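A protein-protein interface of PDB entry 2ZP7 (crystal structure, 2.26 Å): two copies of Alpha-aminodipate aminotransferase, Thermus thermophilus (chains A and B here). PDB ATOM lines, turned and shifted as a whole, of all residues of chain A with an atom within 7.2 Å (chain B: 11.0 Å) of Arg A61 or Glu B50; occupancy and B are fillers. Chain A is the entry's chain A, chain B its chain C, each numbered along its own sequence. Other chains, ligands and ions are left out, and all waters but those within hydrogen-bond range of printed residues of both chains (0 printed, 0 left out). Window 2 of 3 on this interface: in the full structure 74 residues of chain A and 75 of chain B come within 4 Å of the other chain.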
ATOM      1  N   ALA A  53      -4.565 -15.591 -22.784  1.00  0.00           N
ATOM      2  CA  ALA A  53      -3.469 -15.834 -21.840  1.00  0.00           C
ATOM      3  C   ALA A  53      -3.067 -14.530 -21.178  1.00  0.00           C
ATOM      4  O   ALA A  53      -3.048 -14.433 -19.962  1.00  0.00           O
ATOM      5  CB  ALA A  53      -2.277 -16.445 -22.552  1.00  0.00           C
ATOM      6  N   GLU A  54      -2.781 -13.520 -21.998  1.00  0.00           N
ATOM      7  CA  GLU A  54      -2.420 -12.183 -21.527  1.00  0.00           C
ATOM      8  C   GLU A  54      -3.495 -11.569 -20.620  1.00  0.00           C
ATOM      9  O   GLU A  54      -3.185 -11.088 -19.535  1.00  0.00           O
ATOM     10  CB  GLU A  54      -2.123 -11.259 -22.723  1.00  0.00           C
ATOM     11  CG  GLU A  54      -1.524  -9.890 -22.380  1.00  0.00           C
ATOM     12  CD  GLU A  54      -2.501  -8.916 -21.723  1.00  0.00           C
ATOM     13  OE1 GLU A  54      -2.128  -8.295 -20.702  1.00  0.00           O
ATOM     14  OE2 GLU A  54      -3.646  -8.761 -22.209  1.00  0.00           O
ATOM     15  N   ALA A  55      -4.743 -11.563 -21.073  1.00  0.00           N
ATOM     16  CA  ALA A  55      -5.835 -10.952 -20.294  1.00  0.00           C
ATOM     17  C   ALA A  55      -6.147 -11.695 -18.994  1.00  0.00           C
ATOM     18  O   ALA A  55      -6.372 -11.073 -17.968  1.00  0.00           O
ATOM     19  CB  ALA A  55      -7.089 -10.811 -21.145  1.00  0.00           C
ATOM     20  N   ALA A  56      -6.140 -13.025 -19.039  1.00  0.00           N
ATOM     21  CA  ALA A  56      -6.445 -13.847 -17.867  1.00  0.00           C
ATOM     22  C   ALA A  56      -5.406 -13.688 -16.740  1.00  0.00           C
ATOM     23  O   ALA A  56      -5.777 -13.583 -15.571  1.00  0.00           O
ATOM     24  CB  ALA A  56      -6.609 -15.339 -18.268  1.00  0.00           C
ATOM     25  N   ALA A  57      -4.117 -13.688 -17.104  1.00  0.00           N
ATOM     26  CA  ALA A  57      -3.035 -13.421 -16.159  1.00  0.00           C
ATOM     27  C   ALA A  57      -3.208 -12.064 -15.477  1.00  0.00           C
ATOM     28  O   ALA A  57      -3.152 -11.971 -14.244  1.00  0.00           O
ATOM     29  CB  ALA A  57      -1.654 -13.514 -16.849  1.00  0.00           C
ATOM     30  N   ARG A  58      -3.439 -11.034 -16.285  1.00  0.00           N
ATOM     31  CA  ARG A  58      -3.655  -9.673 -15.803  1.00  0.00           C
ATOM     32  C   ARG A  58      -4.876  -9.531 -14.888  1.00  0.00           C
ATOM     33  O   ARG A  58      -4.848  -8.760 -13.926  1.00  0.00           O
ATOM     34  CB  ARG A  58      -3.770  -8.717 -16.992  1.00  0.00           C
ATOM     35  CG  ARG A  58      -4.119  -7.262 -16.626  1.00  0.00           C
ATOM     36  CD  ARG A  58      -3.823  -6.280 -17.787  1.00  0.00           C
ATOM     37  NE  ARG A  58      -4.297  -6.780 -19.072  1.00  0.00           N
ATOM     38  CZ  ARG A  58      -5.496  -6.523 -19.588  1.00  0.00           C
ATOM     39  NH1 ARG A  58      -6.356  -5.746 -18.941  1.00  0.00           N
ATOM     40  NH2 ARG A  58      -5.835  -7.040 -20.763  1.00  0.00           N
ATOM     41  N   ILE A  59      -5.959 -10.243 -15.205  1.00  0.00           N
ATOM     42  CA  ILE A  59      -7.172 -10.184 -14.378  1.00  0.00           C
ATOM     43  C   ILE A  59      -6.833 -10.807 -13.038  1.00  0.00           C
ATOM     44  O   ILE A  59      -7.145 -10.256 -11.996  1.00  0.00           O
ATOM     45  CB  ILE A  59      -8.374 -10.959 -15.007  1.00  0.00           C
ATOM     46  CG1 ILE A  59      -8.968 -10.190 -16.203  1.00  0.00           C
ATOM     47  CG2 ILE A  59      -9.445 -11.219 -13.955  1.00  0.00           C
ATOM     48  CD1 ILE A  59      -9.710 -11.058 -17.195  1.00  0.00           C
ATOM     49  N   LEU A  60      -6.176 -11.956 -13.080  1.00  0.00           N
ATOM     50  CA  LEU A  60      -5.920 -12.711 -11.874  1.00  0.00           C
ATOM     51  C   LEU A  60      -4.865 -12.023 -10.994  1.00  0.00           C
ATOM     52  O   LEU A  60      -4.999 -11.978  -9.768  1.00  0.00           O
ATOM     53  CB  LEU A  60      -5.582 -14.177 -12.212  1.00  0.00           C
ATOM     54  CG  LEU A  60      -6.795 -15.000 -12.716  1.00  0.00           C
ATOM     55  CD1 LEU A  60      -6.374 -16.233 -13.470  1.00  0.00           C
ATOM     56  CD2 LEU A  60      -7.739 -15.401 -11.553  1.00  0.00           C
ATOM     57  N   ARG A  61      -3.844 -11.447 -11.623  1.00  0.00           N
ATOM     58  CA  ARG A  61      -2.827 -10.724 -10.853  1.00  0.00           C
ATOM     59  C   ARG A  61      -3.379  -9.445 -10.260  1.00  0.00           C
ATOM     60  O   ARG A  61      -3.086  -9.120  -9.115  1.00  0.00           O
ATOM     61  CB  ARG A  61      -1.567 -10.447 -11.682  1.00  0.00           C
ATOM     62  CG  ARG A  61      -0.695 -11.686 -11.858  1.00  0.00           C
ATOM     63  CD  ARG A  61       0.553 -11.455 -12.725  1.00  0.00           C
ATOM     64  NE  ARG A  61       1.413 -12.646 -12.717  1.00  0.00           N
ATOM     65  CZ  ARG A  61       1.637 -13.432 -13.773  1.00  0.00           C
ATOM     66  NH1 ARG A  61       1.085 -13.151 -14.950  1.00  0.00           N
ATOM     67  NH2 ARG A  61       2.435 -14.496 -13.664  1.00  0.00           N
ATOM     68  N   GLU A  62      -4.211  -8.740 -11.022  1.00  0.00           N
ATOM     69  CA  GLU A  62      -4.611  -7.382 -10.622  1.00  0.00           C
ATOM     70  C   GLU A  62      -5.995  -7.264 -10.021  1.00  0.00           C
ATOM     71  O   GLU A  62      -6.265  -6.349  -9.242  1.00  0.00           O
ATOM     72  CB  GLU A  62      -4.437  -6.416 -11.792  1.00  0.00           C
ATOM     73  CG  GLU A  62      -2.955  -6.176 -12.082  1.00  0.00           C
ATOM     74  CD  GLU A  62      -2.678  -5.641 -13.469  1.00  0.00           C
ATOM     75  OE1 GLU A  62      -1.528  -5.840 -13.926  1.00  0.00           O
ATOM     76  OE2 GLU A  62      -3.584  -5.016 -14.083  1.00  0.00           O
ATOM     77  N   LYS A  63      -6.856  -8.210 -10.377  1.00  0.00           N
ATOM     78  CA  LYS A  63      -8.252  -8.202  -9.963  1.00  0.00           C
ATOM     79  C   LYS A  63      -8.625  -9.586  -9.425  1.00  0.00           C
ATOM     80  O   LYS A  63      -9.796  -9.975  -9.410  1.00  0.00           O
ATOM     81  CB  LYS A  63      -9.142  -7.828 -11.156  1.00  0.00           C
ATOM     82  CG  LYS A  63      -9.219  -6.338 -11.438  1.00  0.00           C
ATOM     83  CD  LYS A  63      -9.791  -6.104 -12.829  1.00  0.00           C
ATOM     84  CE  LYS A  63     -10.027  -4.612 -13.106  1.00  0.00           C
ATOM     85  NZ  LYS A  63     -10.238  -4.393 -14.581  1.00  0.00           N
ATOM     86  N   GLY A  64      -7.613 -10.328  -8.988  1.00  0.00           N
ATOM     87  CA  GLY A  64      -7.820 -11.691  -8.534  1.00  0.00           C
ATOM     88  C   GLY A  64      -8.817 -11.820  -7.399  1.00  0.00           C
ATOM     89  O   GLY A  64      -9.470 -12.856  -7.277  1.00  0.00           O
ATOM     90  N   GLU A  65      -8.942 -10.782  -6.571  1.00  0.00           N
ATOM     91  CA  GLU A  65      -9.891 -10.811  -5.471  1.00  0.00           C
ATOM     92  C   GLU A  65     -11.362 -10.734  -5.926  1.00  0.00           C
ATOM     93  O   GLU A  65     -12.215 -11.380  -5.337  1.00  0.00           O
ATOM     94  CB  GLU A  65      -9.527  -9.794  -4.371  1.00  0.00           C
ATOM     95  CG  GLU A  65      -9.651  -8.293  -4.751  1.00  0.00           C
ATOM     96  CD  GLU A  65      -8.870  -7.897  -6.007  1.00  0.00           C
ATOM     97  OE1 GLU A  65      -9.538  -7.398  -6.947  1.00  0.00           O
ATOM     98  OE2 GLU A  65      -7.620  -8.090  -6.053  1.00  0.00           O
ATOM     99  N   LEU A  68     -11.928 -14.217  -8.273  1.00  0.00           N
ATOM    100  CA  LEU A  68     -11.874 -15.491  -7.545  1.00  0.00           C
ATOM    101  C   LEU A  68     -12.961 -15.623  -6.464  1.00  0.00           C
ATOM    102  O   LEU A  68     -13.177 -16.712  -5.922  1.00  0.00           O
ATOM    103  CB  LEU A  68     -10.479 -15.677  -6.912  1.00  0.00           C
ATOM    104  CG  LEU A  68      -9.399 -16.561  -7.572  1.00  0.00           C
ATOM    105  CD1 LEU A  68      -9.674 -16.933  -9.035  1.00  0.00           C
ATOM    106  CD2 LEU A  68      -7.950 -16.043  -7.378  1.00  0.00           C
ATOM    107  N   PRO B  44     -10.197 -13.824   1.343  1.00  0.00           N
ATOM    108  CA  PRO B  44      -9.453 -13.461   0.150  1.00  0.00           C
ATOM    109  C   PRO B  44      -7.945 -13.626   0.320  1.00  0.00           C
ATOM    110  O   PRO B  44      -7.249 -13.930  -0.655  1.00  0.00           O
ATOM    111  CB  PRO B  44      -9.838 -11.990  -0.088  1.00  0.00           C
ATOM    112  CG  PRO B  44     -10.328 -11.503   1.211  1.00  0.00           C
ATOM    113  CD  PRO B  44     -10.961 -12.682   1.877  1.00  0.00           C
ATOM    114  N   GLU B  45      -7.451 -13.466   1.547  1.00  0.00           N
ATOM    115  CA  GLU B  45      -6.028 -13.677   1.838  1.00  0.00           C
ATOM    116  C   GLU B  45      -5.516 -15.061   1.405  1.00  0.00           C
ATOM    117  O   GLU B  45      -4.319 -15.221   1.144  1.00  0.00           O
ATOM    118  CB  GLU B  45      -5.700 -13.407   3.323  1.00  0.00           C
ATOM    119  CG  GLU B  45      -6.488 -14.209   4.327  1.00  0.00           C
ATOM    120  CD  GLU B  45      -7.700 -13.442   4.861  1.00  0.00           C
ATOM    121  OE1 GLU B  45      -7.793 -13.285   6.098  1.00  0.00           O
ATOM    122  OE2 GLU B  45      -8.550 -12.986   4.056  1.00  0.00           O
ATOM    123  N   LEU B  46      -6.424 -16.035   1.323  1.00  0.00           N
ATOM    124  CA  LEU B  46      -6.113 -17.408   0.907  1.00  0.00           C
ATOM    125  C   LEU B  46      -6.034 -17.585  -0.611  1.00  0.00           C
ATOM    126  O   LEU B  46      -5.507 -18.584  -1.081  1.00  0.00           O
ATOM    127  CB  LEU B  46      -7.164 -18.372   1.478  1.00  0.00           C
ATOM    128  CG  LEU B  46      -6.960 -19.467   2.553  1.00  0.00           C
ATOM    129  CD1 LEU B  46      -5.669 -19.423   3.342  1.00  0.00           C
ATOM    130  CD2 LEU B  46      -8.163 -19.554   3.498  1.00  0.00           C
ATOM    131  N   PHE B  47      -6.578 -16.638  -1.376  1.00  0.00           N
ATOM    132  CA  PHE B  47      -6.556 -16.705  -2.846  1.00  0.00           C
ATOM    133  C   PHE B  47      -5.130 -16.773  -3.425  1.00  0.00           C
ATOM    134  O   PHE B  47      -4.312 -15.890  -3.186  1.00  0.00           O
ATOM    135  CB  PHE B  47      -7.297 -15.509  -3.459  1.00  0.00           C
ATOM    136  CG  PHE B  47      -8.803 -15.490  -3.196  1.00  0.00           C
ATOM    137  CD1 PHE B  47      -9.491 -16.632  -2.784  1.00  0.00           C
ATOM    138  CD2 PHE B  47      -9.531 -14.322  -3.413  1.00  0.00           C
ATOM    139  CE1 PHE B  47     -10.853 -16.589  -2.544  1.00  0.00           C
ATOM    140  CE2 PHE B  47     -10.903 -14.287  -3.206  1.00  0.00           C
ATOM    141  CZ  PHE B  47     -11.565 -15.407  -2.763  1.00  0.00           C
ATOM    142  N   PRO B  48      -4.833 -17.818  -4.211  1.00  0.00           N
ATOM    143  CA  PRO B  48      -3.506 -17.889  -4.811  1.00  0.00           C
ATOM    144  C   PRO B  48      -3.486 -17.185  -6.161  1.00  0.00           C
ATOM    145  O   PRO B  48      -3.471 -17.855  -7.187  1.00  0.00           O
ATOM    146  CB  PRO B  48      -3.308 -19.388  -4.999  1.00  0.00           C
ATOM    147  CG  PRO B  48      -4.699 -19.903  -5.309  1.00  0.00           C
ATOM    148  CD  PRO B  48      -5.673 -18.972  -4.583  1.00  0.00           C
ATOM    149  N   LYS B  49      -3.498 -15.854  -6.150  1.00  0.00           N
ATOM    150  CA  LYS B  49      -3.691 -15.046  -7.362  1.00  0.00           C
ATOM    151  C   LYS B  49      -2.555 -15.215  -8.370  1.00  0.00           C
ATOM    152  O   LYS B  49      -2.797 -15.409  -9.562  1.00  0.00           O
ATOM    153  CB  LYS B  49      -3.862 -13.558  -7.000  1.00  0.00           C
ATOM    154  CG  LYS B  49      -5.217 -13.219  -6.358  1.00  0.00           C
ATOM    155  CD  LYS B  49      -5.363 -11.741  -6.012  1.00  0.00           C
ATOM    156  CE  LYS B  49      -4.418 -11.302  -4.871  1.00  0.00           C
ATOM    157  NZ  LYS B  49      -4.981 -10.144  -4.127  1.00  0.00           N
ATOM    158  N   GLU B  50      -1.324 -15.149  -7.864  1.00  0.00           N
ATOM    159  CA  GLU B  50      -0.118 -15.283  -8.674  1.00  0.00           C
ATOM    160  C   GLU B  50       0.066 -16.679  -9.269  1.00  0.00           C
ATOM    161  O   GLU B  50       0.399 -16.805 -10.449  1.00  0.00           O
ATOM    162  CB  GLU B  50       1.121 -14.831  -7.882  1.00  0.00           C
ATOM    163  CG  GLU B  50       2.429 -14.827  -8.680  1.00  0.00           C
ATOM    164  CD  GLU B  50       2.421 -13.884  -9.893  1.00  0.00           C
ATOM    165  OE1 GLU B  50       1.900 -12.737  -9.792  1.00  0.00           O
ATOM    166  OE2 GLU B  50       2.958 -14.302 -10.946  1.00  0.00           O
ATOM    167  N   GLU B  51      -0.157 -17.729  -8.483  1.00  0.00           N
ATOM    168  CA  GLU B  51      -0.110 -19.071  -9.062  1.00  0.00           C
ATOM    169  C   GLU B  51      -1.222 -19.176 -10.088  1.00  0.00           C
ATOM    170  O   GLU B  51      -1.009 -19.690 -11.190  1.00  0.00           O
ATOM    171  CB  GLU B  51      -0.332 -20.161  -8.025  1.00  0.00           C
ATOM    172  CG  GLU B  51       0.695 -20.307  -6.954  1.00  0.00           C
ATOM    173  CD  GLU B  51       0.276 -21.388  -5.974  1.00  0.00           C
ATOM    174  OE1 GLU B  51      -0.338 -21.060  -4.924  1.00  0.00           O
ATOM    175  OE2 GLU B  51       0.512 -22.573  -6.288  1.00  0.00           O
ATOM    176  N   ALA B  52      -2.411 -18.689  -9.713  1.00  0.00           N
ATOM    177  CA  ALA B  52      -3.592 -18.746 -10.584  1.00  0.00           C
ATOM    178  C   ALA B  52      -3.321 -18.041 -11.912  1.00  0.00           C
ATOM    179  O   ALA B  52      -3.643 -18.563 -12.976  1.00  0.00           O
ATOM    180  CB  ALA B  52      -4.800 -18.148  -9.895  1.00  0.00           C
ATOM    181  N   ALA B  53      -2.719 -16.858 -11.829  1.00  0.00           N
ATOM    182  CA  ALA B  53      -2.398 -16.044 -13.003  1.00  0.00           C
ATOM    183  C   ALA B  53      -1.434 -16.775 -13.943  1.00  0.00           C
ATOM    184  O   ALA B  53      -1.682 -16.855 -15.135  1.00  0.00           O
ATOM    185  CB  ALA B  53      -1.826 -14.708 -12.572  1.00  0.00           C
ATOM    186  N   GLU B  54      -0.358 -17.319 -13.389  1.00  0.00           N
ATOM    187  CA  GLU B  54       0.635 -18.104 -14.136  1.00  0.00           C
ATOM    188  C   GLU B  54       0.049 -19.398 -14.737  1.00  0.00           C
ATOM    189  O   GLU B  54       0.271 -19.680 -15.913  1.00  0.00           O
ATOM    190  CB  GLU B  54       1.849 -18.422 -13.240  1.00  0.00           C
ATOM    191  CG  GLU B  54       2.927 -19.341 -13.876  1.00  0.00           C
ATOM    192  CD  GLU B  54       2.557 -20.830 -13.877  1.00  0.00           C
ATOM    193  OE1 GLU B  54       3.037 -21.572 -14.770  1.00  0.00           O
ATOM    194  OE2 GLU B  54       1.789 -21.264 -12.985  1.00  0.00           O
ATOM    195  N   ALA B  55      -0.678 -20.182 -13.933  1.00  0.00           N
ATOM    196  CA  ALA B  55      -1.358 -21.379 -14.440  1.00  0.00           C
ATOM    197  C   ALA B  55      -2.322 -21.078 -15.597  1.00  0.00           C
ATOM    198  O   ALA B  55      -2.334 -21.793 -16.598  1.00  0.00           O
ATOM    199  CB  ALA B  55      -2.080 -22.100 -13.323  1.00  0.00           C
ATOM    200  N   ALA B  56      -3.095 -19.997 -15.478  1.00  0.00           N
ATOM    201  CA  ALA B  56      -4.091 -19.642 -16.493  1.00  0.00           C
ATOM    202  C   ALA B  56      -3.475 -19.304 -17.850  1.00  0.00           C
ATOM    203  O   ALA B  56      -3.956 -19.788 -18.886  1.00  0.00           O
ATOM    204  CB  ALA B  56      -4.986 -18.508 -16.008  1.00  0.00           C
ATOM    205  N   ALA B  57      -2.436 -18.466 -17.839  1.00  0.00           N
ATOM    206  CA  ALA B  57      -1.704 -18.083 -19.065  1.00  0.00           C
ATOM    207  C   ALA B  57      -1.063 -19.282 -19.742  1.00  0.00           C
ATOM    208  O   ALA B  57      -1.124 -19.408 -20.960  1.00  0.00           O
ATOM    209  CB  ALA B  57      -0.642 -17.030 -18.762  1.00  0.00           C
ATOM    210  N   ARG B  58      -0.464 -20.160 -18.940  1.00  0.00           N
ATOM    211  CA  ARG B  58       0.156 -21.372 -19.437  1.00  0.00           C
ATOM    212  C   ARG B  58      -0.890 -22.273 -20.086  1.00  0.00           C
ATOM    213  O   ARG B  58      -0.650 -22.807 -21.171  1.00  0.00           O
ATOM    214  CB  ARG B  58       0.849 -22.115 -18.298  1.00  0.00           C
ATOM    215  CG  ARG B  58       2.053 -22.941 -18.721  1.00  0.00           C
ATOM    216  CD  ARG B  58       2.480 -23.979 -17.667  1.00  0.00           C
ATOM    217  NE  ARG B  58       2.209 -23.556 -16.288  1.00  0.00           N
ATOM    218  CZ  ARG B  58       1.479 -24.252 -15.418  1.00  0.00           C
ATOM    219  NH1 ARG B  58       0.957 -25.419 -15.777  1.00  0.00           N
ATOM    220  NH2 ARG B  58       1.281 -23.791 -14.183  1.00  0.00           N
ATOM    221  N   ILE B  59      -2.044 -22.431 -19.424  1.00  0.00           N
ATOM    222  CA  ILE B  59      -3.174 -23.225 -19.953  1.00  0.00           C
ATOM    223  C   ILE B  59      -3.642 -22.662 -21.301  1.00  0.00           C
ATOM    224  O   ILE B  59      -3.858 -23.395 -22.268  1.00  0.00           O
ATOM    225  CB  ILE B  59      -4.391 -23.274 -18.938  1.00  0.00           C
ATOM    226  CG1 ILE B  59      -4.072 -24.167 -17.726  1.00  0.00           C
ATOM    227  CG2 ILE B  59      -5.669 -23.765 -19.617  1.00  0.00           C
ATOM    228  CD1 ILE B  59      -4.909 -23.860 -16.473  1.00  0.00           C
ATOM    229  N   LEU B  60      -3.805 -21.354 -21.355  1.00  0.00           N
ATOM    230  CA  LEU B  60      -4.358 -20.725 -22.543  1.00  0.00           C
ATOM    231  C   LEU B  60      -3.330 -20.697 -23.683  1.00  0.00           C
ATOM    232  O   LEU B  60      -3.697 -20.877 -24.841  1.00  0.00           O
ATOM    233  CB  LEU B  60      -4.948 -19.348 -22.216  1.00  0.00           C
ATOM    234  CG  LEU B  60      -6.290 -19.397 -21.455  1.00  0.00           C
ATOM    235  CD1 LEU B  60      -6.723 -18.046 -20.906  1.00  0.00           C
ATOM    236  CD2 LEU B  60      -7.401 -19.949 -22.327  1.00  0.00           C
ATOM    237  N   ARG B  61      -2.049 -20.532 -23.351  1.00  0.00           N
ATOM    238  CA  ARG B  61      -0.967 -20.651 -24.352  1.00  0.00           C
ATOM    239  C   ARG B  61      -0.699 -22.071 -24.872  1.00  0.00           C
ATOM    240  O   ARG B  61      -0.504 -22.260 -26.066  1.00  0.00           O
ATOM    241  CB  ARG B  61       0.333 -20.036 -23.840  1.00  0.00           C
ATOM    242  CG  ARG B  61       0.373 -18.562 -24.066  1.00  0.00           C
ATOM    243  CD  ARG B  61       1.647 -17.949 -23.539  1.00  0.00           C
ATOM    244  NE  ARG B  61       1.510 -16.495 -23.490  1.00  0.00           N
ATOM    245  CZ  ARG B  61       1.539 -15.770 -22.380  1.00  0.00           C
ATOM    246  NH1 ARG B  61       1.722 -16.357 -21.207  1.00  0.00           N
ATOM    247  NH2 ARG B  61       1.399 -14.447 -22.458  1.00  0.00           N
ATOM    248  N   LEU B 240     -10.364 -23.196  -2.220  1.00  0.00           N
ATOM    249  CA  LEU B 240      -9.569 -22.610  -3.276  1.00  0.00           C
ATOM    250  C   LEU B 240     -10.148 -21.308  -3.805  1.00  0.00           C
ATOM    251  O   LEU B 240      -9.488 -20.257  -3.709  1.00  0.00           O
ATOM    252  CB  LEU B 240      -9.446 -23.593  -4.425  1.00  0.00           C
ATOM    253  CG  LEU B 240      -8.159 -23.688  -5.245  1.00  0.00           C
ATOM    254  CD1 LEU B 240      -8.519 -23.904  -6.702  1.00  0.00           C
ATOM    255  CD2 LEU B 240      -7.183 -22.502  -5.058  1.00  0.00           C
ATOM    256  N   LEU B 277      -7.779 -25.009 -14.561  1.00  0.00           N
ATOM    257  CA  LEU B 277      -7.121 -24.121 -13.615  1.00  0.00           C
ATOM    258  C   LEU B 277      -7.106 -24.675 -12.186  1.00  0.00           C
ATOM    259  O   LEU B 277      -6.066 -24.654 -11.505  1.00  0.00           O
ATOM    260  CB  LEU B 277      -7.743 -22.729 -13.683  1.00  0.00           C
ATOM    261  CG  LEU B 277      -7.181 -21.580 -12.834  1.00  0.00           C
ATOM    262  CD1 LEU B 277      -5.710 -21.261 -13.172  1.00  0.00           C
ATOM    263  CD2 LEU B 277      -8.069 -20.361 -13.071  1.00  0.00           C
ATOM    264  N   GLU B 280      -4.580 -27.695 -12.228  1.00  0.00           N
ATOM    265  CA  GLU B 280      -3.213 -27.193 -12.198  1.00  0.00           C
ATOM    266  C   GLU B 280      -2.813 -26.682 -10.810  1.00  0.00           C
ATOM    267  O   GLU B 280      -1.671 -26.873 -10.377  1.00  0.00           O
ATOM    268  CB  GLU B 280      -3.002 -26.086 -13.226  1.00  0.00           C
ATOM    269  CG  GLU B 280      -2.947 -26.575 -14.678  1.00  0.00           C
ATOM    270  CD  GLU B 280      -1.769 -27.513 -14.957  1.00  0.00           C
ATOM    271  OE1 GLU B 280      -0.613 -27.175 -14.590  1.00  0.00           O
ATOM    272  OE2 GLU B 280      -2.012 -28.593 -15.547  1.00  0.00           O
ATOM    273  N   LEU B 281      -3.761 -26.041 -10.115  1.00  0.00           N
ATOM    274  CA  LEU B 281      -3.468 -25.434  -8.814  1.00  0.00           C
ATOM    275  C   LEU B 281      -3.338 -26.446  -7.704  1.00  0.00           C
ATOM    276  O   LEU B 281      -2.692 -26.183  -6.687  1.00  0.00           O
ATOM    277  CB  LEU B 281      -4.515 -24.382  -8.447  1.00  0.00           C
ATOM    278  CG  LEU B 281      -4.286 -23.048  -9.170  1.00  0.00           C
ATOM    279  CD1 LEU B 281      -5.515 -22.130  -9.170  1.00  0.00           C
ATOM    280  CD2 LEU B 281      -3.054 -22.332  -8.627  1.00  0.00           C
ATOM    281  N   ARG B 289      -1.725 -26.856   1.262  1.00  0.00           N
ATOM    282  CA  ARG B 289      -2.663 -25.750   1.078  1.00  0.00           C
ATOM    283  C   ARG B 289      -3.843 -25.835   2.057  1.00  0.00           C
ATOM    284  O   ARG B 289      -4.248 -24.832   2.628  1.00  0.00           O
ATOM    285  CB  ARG B 289      -3.158 -25.666  -0.369  1.00  0.00           C
ATOM    286  CG  ARG B 289      -4.095 -24.491  -0.619  1.00  0.00           C
ATOM    287  CD  ARG B 289      -4.568 -24.385  -2.065  1.00  0.00           C
ATOM    288  NE  ARG B 289      -3.459 -24.240  -3.007  1.00  0.00           N
ATOM    289  CZ  ARG B 289      -2.748 -23.124  -3.195  1.00  0.00           C
ATOM    290  NH1 ARG B 289      -3.012 -22.008  -2.507  1.00  0.00           N
ATOM    291  NH2 ARG B 289      -1.755 -23.128  -4.080  1.00  0.00           N
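Printed residues of chain B within 4 Å of Ala A56: Leu B60.
Of chain B, only Lys B49 (3.4 Å), Ala B52 (3.6 Å), Ala B53 (3.8 Å) and Ala B56 (3.7 Å) come within 4 Å of Leu A60.
Of the printed residues of chain B, Arg A61 touches Glu B50, Ala B53 and Glu B54.
Printed residues of chain B within 4 Å of Glu A65: Phe B47 (3.8 Å) and Lys B49 (3.7 Å).
Of the printed residues of chain A, Ala B52 touches Leu A60 (3.6 Å).
Ala B55 touches none of the printed residues of chain A.
Printed residues of chain A within 4 Å of Ala B56: Leu A60 (3.7 Å).
Leu B240 touches none of the printed residues of chain A.
The nearest printed residue of chain B that does not touch Arg A61 is Lys B49 (4.6 Å).
The nearest residue of chain A that does not touch Glu B50 is Leu A60 (5.2 Å).
Ala A53 touches Ala B57, and with the chains exchanged Ala A57 touches Ala B53.
Ala A53 touches Leu B60, and with the chains exchanged Leu A60 touches Ala B53.
Ala A53 touches Arg B61, and with the chains exchanged Arg A61 touches Ala B53.
Ala A56 touches Leu B60, and with the chains exchanged Leu A60 touches Ala B56.
Positions printed for both chains: 53, 54, 55, 56, 57, 58, 59, 60 and 61.
Of the 16 pairs that touch across the chains among the printed residues, 8 have their exchanged pair printed and touching as well.
N of Gly A64 is in hydrogen-bond range of O of Ile A59 (3.0 Å).
The side-chain carboxylate (OE1) of Glu B54 is in salt-bridge range of the guanidinium group (NE) of Arg B58 (2.6 Å).
Among the printed residues, merely in contact across the chains: Arg A61 with Ala B53 (3.3 Å), Leu A60 with Lys B49 (3.4 Å), Ala A57 with Ala B53 (3.5 Å), Gly A64 with Lys B49 (3.5 Å), Ala A53 with Ala B57 (3.6 Å), Leu A60 with Ala B52 (3.6 Å), Leu A60 with Ala B56 (3.7 Å), Ala A53 with Arg B61 (3.7 Å), Ala A53 with Leu B60 (3.8 Å), Leu A60 with Ala B53 (3.8 Å), Leu A68 with Phe B47 (3.8 Å), Ala A56 with Leu B60 (3.8 Å), Glu A65 with Phe B47 (3.8 Å) and Arg A61 with Glu B54 (3.98 Å).
The guanidinium group (NH2) of Arg A61 lies within salt-bridge range of the side-chain carboxylate (OE2) of Glu B50 (2.8 Å).
The side-chain carboxylate (OE2) of Glu A65 is in salt-bridge range of the side-chain amino group (NZ) of Lys B49 (3.9 Å).
Of the 23 printed residues of chain B, 10 touch a printed residue of chain A.
Of the 14 printed residues of chain A, 8 touch a printed residue of chain B.
Along chain A the printed residues that touch a printed residue of chain B span positions 53 to 68.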
